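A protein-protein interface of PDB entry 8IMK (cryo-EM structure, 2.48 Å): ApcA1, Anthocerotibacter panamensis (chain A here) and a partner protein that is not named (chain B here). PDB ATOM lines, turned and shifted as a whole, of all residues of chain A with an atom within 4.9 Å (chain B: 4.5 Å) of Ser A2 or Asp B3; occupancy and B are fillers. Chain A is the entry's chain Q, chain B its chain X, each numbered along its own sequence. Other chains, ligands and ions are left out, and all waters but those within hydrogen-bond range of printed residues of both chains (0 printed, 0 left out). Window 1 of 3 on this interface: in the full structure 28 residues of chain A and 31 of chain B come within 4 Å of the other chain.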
ATOM      1  N   SER A   2     -10.799   5.173 -25.040  1.00  0.00           N
ATOM      2  CA  SER A   2     -12.174   5.618 -25.202  1.00  0.00           C
ATOM      3  C   SER A   2     -12.747   6.074 -23.871  1.00  0.00           C
ATOM      4  O   SER A   2     -12.210   5.756 -22.818  1.00  0.00           O
ATOM      5  CB  SER A   2     -13.030   4.501 -25.792  1.00  0.00           C
ATOM      6  OG  SER A   2     -14.228   5.007 -26.342  1.00  0.00           O
ATOM      7  N   ALA A   3     -13.835   6.842 -23.925  1.00  0.00           N
ATOM      8  CA  ALA A   3     -14.582   7.140 -22.709  1.00  0.00           C
ATOM      9  C   ALA A   3     -15.168   5.868 -22.109  1.00  0.00           C
ATOM     10  O   ALA A   3     -15.127   5.663 -20.888  1.00  0.00           O
ATOM     11  CB  ALA A   3     -15.679   8.154 -23.016  1.00  0.00           C
ATOM     12  N   ILE A   4     -15.695   4.991 -22.964  1.00  0.00           N
ATOM     13  CA  ILE A   4     -16.244   3.721 -22.510  1.00  0.00           C
ATOM     14  C   ILE A   4     -15.162   2.860 -21.877  1.00  0.00           C
ATOM     15  O   ILE A   4     -15.373   2.256 -20.822  1.00  0.00           O
ATOM     16  CB  ILE A   4     -16.929   2.997 -23.681  1.00  0.00           C
ATOM     17  CG1 ILE A   4     -18.278   3.641 -23.985  1.00  0.00           C
ATOM     18  CG2 ILE A   4     -17.094   1.523 -23.378  1.00  0.00           C
ATOM     19  CD1 ILE A   4     -18.967   3.042 -25.167  1.00  0.00           C
ATOM     20  N   THR A   5     -13.994   2.777 -22.514  1.00  0.00           N
ATOM     21  CA  THR A   5     -12.908   1.970 -21.971  1.00  0.00           C
ATOM     22  C   THR A   5     -12.444   2.498 -20.624  1.00  0.00           C
ATOM     23  O   THR A   5     -12.187   1.720 -19.701  1.00  0.00           O
ATOM     24  CB  THR A   5     -11.744   1.929 -22.956  1.00  0.00           C
ATOM     25  OG1 THR A   5     -12.178   1.348 -24.188  1.00  0.00           O
ATOM     26  CG2 THR A   5     -10.589   1.128 -22.389  1.00  0.00           C
ATOM     27  N   LYS A   6     -12.333   3.816 -20.488  1.00  0.00           N
ATOM     28  CA  LYS A   6     -11.915   4.392 -19.218  1.00  0.00           C
ATOM     29  C   LYS A   6     -12.932   4.088 -18.124  1.00  0.00           C
ATOM     30  O   LYS A   6     -12.562   3.641 -17.030  1.00  0.00           O
ATOM     31  CB  LYS A   6     -11.691   5.895 -19.401  1.00  0.00           C
ATOM     32  CG  LYS A   6     -11.082   6.639 -18.231  1.00  0.00           C
ATOM     33  CD  LYS A   6     -12.125   7.208 -17.291  1.00  0.00           C
ATOM     34  CE  LYS A   6     -11.465   8.005 -16.181  1.00  0.00           C
ATOM     35  NZ  LYS A   6     -12.463   8.545 -15.223  1.00  0.00           N
ATOM     36  N   TYR A  29     -21.206  10.511 -24.123  1.00  0.00           N
ATOM     37  CA  TYR A  29     -20.313  10.211 -25.239  1.00  0.00           C
ATOM     38  C   TYR A  29     -21.083   9.642 -26.428  1.00  0.00           C
ATOM     39  O   TYR A  29     -20.891  10.072 -27.577  1.00  0.00           O
ATOM     40  CB  TYR A  29     -19.223   9.247 -24.772  1.00  0.00           C
ATOM     41  CG  TYR A  29     -18.425   8.596 -25.871  1.00  0.00           C
ATOM     42  CD1 TYR A  29     -17.592   9.345 -26.690  1.00  0.00           C
ATOM     43  CD2 TYR A  29     -18.482   7.231 -26.074  1.00  0.00           C
ATOM     44  CE1 TYR A  29     -16.863   8.756 -27.687  1.00  0.00           C
ATOM     45  CE2 TYR A  29     -17.752   6.632 -27.070  1.00  0.00           C
ATOM     46  CZ  TYR A  29     -16.944   7.401 -27.873  1.00  0.00           C
ATOM     47  OH  TYR A  29     -16.206   6.814 -28.870  1.00  0.00           O
ATOM     48  N   ALA A  98     -12.664   8.992 -30.269  1.00  0.00           N
ATOM     49  CA  ALA A  98     -12.661   8.117 -29.105  1.00  0.00           C
ATOM     50  C   ALA A  98     -13.125   8.842 -27.853  1.00  0.00           C
ATOM     51  O   ALA A  98     -13.380   8.208 -26.825  1.00  0.00           O
ATOM     52  CB  ALA A  98     -11.267   7.534 -28.893  1.00  0.00           C
ATOM     53  N   ASP A 100     -11.542  10.603 -25.782  1.00  0.00           N
ATOM     54  CA  ASP A 100     -10.528  10.821 -24.764  1.00  0.00           C
ATOM     55  C   ASP A 100      -9.175  10.841 -25.457  1.00  0.00           C
ATOM     56  O   ASP A 100      -9.081  10.753 -26.681  1.00  0.00           O
ATOM     57  CB  ASP A 100     -10.592   9.757 -23.666  1.00  0.00           C
ATOM     58  CG  ASP A 100      -9.941   8.467 -24.070  1.00  0.00           C
ATOM     59  OD1 ASP A 100     -10.173   8.013 -25.207  1.00  0.00           O
ATOM     60  OD2 ASP A 100      -9.201   7.900 -23.244  1.00  0.00           O
ATOM     61  N   SER A 102      -6.571   8.727 -24.893  1.00  0.00           N
ATOM     62  CA  SER A 102      -5.792   7.494 -24.899  1.00  0.00           C
ATOM     63  C   SER A 102      -5.182   7.185 -26.263  1.00  0.00           C
ATOM     64  O   SER A 102      -3.946   7.080 -26.325  1.00  0.00           O
ATOM     65  CB  SER A 102      -6.639   6.331 -24.360  1.00  0.00           C
ATOM     66  OG  SER A 102      -7.735   6.006 -25.188  1.00  0.00           O
ATOM     67  N   MET B   1      -8.249  -1.637 -22.114  1.00  0.00           N
ATOM     68  CA  MET B   1      -8.992  -2.633 -22.878  1.00  0.00           C
ATOM     69  C   MET B   1      -9.577  -2.034 -24.153  1.00  0.00           C
ATOM     70  O   MET B   1      -9.314  -0.881 -24.481  1.00  0.00           O
ATOM     71  CB  MET B   1     -10.092  -3.245 -22.016  1.00  0.00           C
ATOM     72  CG  MET B   1     -10.981  -2.233 -21.335  1.00  0.00           C
ATOM     73  SD  MET B   1     -12.628  -2.882 -21.039  1.00  0.00           S
ATOM     74  CE  MET B   1     -13.354  -2.719 -22.663  1.00  0.00           C
ATOM     75  N   LEU B   2     -10.360  -2.825 -24.879  1.00  0.00           N
ATOM     76  CA  LEU B   2     -10.847  -2.448 -26.197  1.00  0.00           C
ATOM     77  C   LEU B   2     -12.365  -2.446 -26.235  1.00  0.00           C
ATOM     78  O   LEU B   2     -13.006  -3.382 -25.751  1.00  0.00           O
ATOM     79  CB  LEU B   2     -10.331  -3.401 -27.274  1.00  0.00           C
ATOM     80  CG  LEU B   2      -9.024  -3.105 -27.997  1.00  0.00           C
ATOM     81  CD1 LEU B   2      -7.863  -2.987 -27.030  1.00  0.00           C
ATOM     82  CD2 LEU B   2      -8.770  -4.204 -29.001  1.00  0.00           C
ATOM     83  N   ASP B   3     -12.927  -1.396 -26.816  1.00  0.00           N
ATOM     84  CA  ASP B   3     -14.300  -1.385 -27.279  1.00  0.00           C
ATOM     85  C   ASP B   3     -14.295  -1.332 -28.800  1.00  0.00           C
ATOM     86  O   ASP B   3     -13.247  -1.416 -29.439  1.00  0.00           O
ATOM     87  CB  ASP B   3     -15.087  -0.214 -26.685  1.00  0.00           C
ATOM     88  CG  ASP B   3     -14.376   1.099 -26.843  1.00  0.00           C
ATOM     89  OD1 ASP B   3     -15.057   2.142 -26.878  1.00  0.00           O
ATOM     90  OD2 ASP B   3     -13.133   1.090 -26.917  1.00  0.00           O
ATOM     91  N   ALA B   4     -15.486  -1.205 -29.382  1.00  0.00           N
ATOM     92  CA  ALA B   4     -15.593  -1.242 -30.836  1.00  0.00           C
ATOM     93  C   ALA B   4     -14.852  -0.077 -31.485  1.00  0.00           C
ATOM     94  O   ALA B   4     -14.144  -0.258 -32.485  1.00  0.00           O
ATOM     95  CB  ALA B   4     -17.061  -1.244 -31.248  1.00  0.00           C
ATOM     96  N   VAL B   5     -14.997   1.125 -30.926  1.00  0.00           N
ATOM     97  CA  VAL B   5     -14.369   2.303 -31.515  1.00  0.00           C
ATOM     98  C   VAL B   5     -12.853   2.187 -31.459  1.00  0.00           C
ATOM     99  O   VAL B   5     -12.157   2.509 -32.428  1.00  0.00           O
ATOM    100  CB  VAL B   5     -14.866   3.576 -30.813  1.00  0.00           C
ATOM    101  CG1 VAL B   5     -14.271   4.811 -31.461  1.00  0.00           C
ATOM    102  CG2 VAL B   5     -16.369   3.626 -30.856  1.00  0.00           C
ATOM    103  N   THR B   6     -12.315   1.739 -30.325  1.00  0.00           N
ATOM    104  CA  THR B   6     -10.874   1.542 -30.229  1.00  0.00           C
ATOM    105  C   THR B   6     -10.409   0.428 -31.150  1.00  0.00           C
ATOM    106  O   THR B   6      -9.289   0.471 -31.660  1.00  0.00           O
ATOM    107  CB  THR B   6     -10.464   1.256 -28.788  1.00  0.00           C
ATOM    108  OG1 THR B   6     -11.312   0.241 -28.238  1.00  0.00           O
ATOM    109  CG2 THR B   6     -10.562   2.515 -27.955  1.00  0.00           C
ATOM    110  N   LYS B   7     -11.257  -0.570 -31.391  1.00  0.00           N
ATOM    111  CA  LYS B   7     -10.905  -1.598 -32.363  1.00  0.00           C
ATOM    112  C   LYS B   7     -10.755  -1.000 -33.759  1.00  0.00           C
ATOM    113  O   LYS B   7      -9.784  -1.292 -34.469  1.00  0.00           O
ATOM    114  CB  LYS B   7     -11.953  -2.708 -32.348  1.00  0.00           C
ATOM    115  CG  LYS B   7     -11.682  -3.830 -33.322  1.00  0.00           C
ATOM    116  CD  LYS B   7     -10.448  -4.611 -32.916  1.00  0.00           C
ATOM    117  CE  LYS B   7     -10.249  -5.832 -33.796  1.00  0.00           C
ATOM    118  NZ  LYS B   7      -9.936  -5.445 -35.203  1.00  0.00           N
ATOM    119  N   ALA B  99     -19.162  -2.138 -23.902  1.00  0.00           N
ATOM    120  CA  ALA B  99     -18.053  -1.915 -24.817  1.00  0.00           C
ATOM    121  C   ALA B  99     -18.442  -2.245 -26.250  1.00  0.00           C
ATOM    122  O   ALA B  99     -17.898  -1.670 -27.197  1.00  0.00           O
ATOM    123  CB  ALA B  99     -16.847  -2.741 -24.384  1.00  0.00           C
ATOM    124  N   ASP B 101     -17.850  -5.154 -27.485  1.00  0.00           N
ATOM    125  CA  ASP B 101     -16.763  -6.013 -27.915  1.00  0.00           C
ATOM    126  C   ASP B 101     -16.509  -7.047 -26.831  1.00  0.00           C
ATOM    127  O   ASP B 101     -16.778  -6.806 -25.655  1.00  0.00           O
ATOM    128  CB  ASP B 101     -15.506  -5.178 -28.209  1.00  0.00           C
ATOM    129  CG  ASP B 101     -14.283  -6.026 -28.443  1.00  0.00           C
ATOM    130  OD1 ASP B 101     -14.260  -6.794 -29.427  1.00  0.00           O
ATOM    131  OD2 ASP B 101     -13.335  -5.911 -27.646  1.00  0.00           O
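The side-chain carboxylate (OD1) of Asp B3 is in hydrogen-bond range of the side-chain hydroxyl (OG) of Ser A2 (3.0 Å). The side-chain hydroxyl (OG1) of Thr A5 lies within hydrogen-bond range of the side-chain carboxylate (OD2) of Asp B3 (2.9 Å).
The side-chain hydroxyl of Ser A2 lies close to the backbone carbonyl oxygen of Ala A98 (3.3 Å). The backbone NH of Ser A2 sits at hydrogen-bond distance from the side-chain carboxylate of Asp A100 (2.9 Å). The side-chain hydroxyl (OG) of Ser A102 lies within hydrogen-bond range of the backbone NH (N) of Ser A2. The side-chain hydroxyl of Thr B6 lies within hydrogen-bond range of the side-chain carboxylate of Asp B3, at 2.4 Å. O of Ala B99 sits at hydrogen-bond distance from N of Ala B4 (3.3 Å).
Among the printed residues, pairs that only touch across the chains: Thr A5 with Met B1 (3.2 Å), Tyr A29 with Val B5 (3.8 Å), Ile A4 with Asp B3 (3.8 Å), Ser A2 with Thr B6 (3.8 Å) and Ile A4 with Ala B99 (3.8 Å).
Ser A2 touches just these residues of chain B: Asp B3 (3.0 Å) and Thr B6 (3.8 Å). Printed residues of chain B within 4 Å of Ile A4: Asp B3 and Ala B99. Of the printed residues of chain B, Tyr A29 touches Val B5. Asp A100 touches none of the printed residues of chain B. Ser A102 touches none of the printed residues of chain B. Of chain A, only Ser A2, Ile A4 and Thr A5 come within 4 Å of Asp B3. The nearest printed residue of chain B that does not touch Ser A2 is Val B5 (4.7 Å). The nearest printed residue of chain B that does not touch Tyr A29 is Asp B3 (5.2 Å).
Of the 9 printed residues of chain A, 4 touch a printed residue of chain B. Hydrophobic or aromatic side chains of chain A that line the printed part of chain B: Ile A4 and Tyr A29. Along chain A the printed residues that touch a printed residue of chain B span positions 2 to 29.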
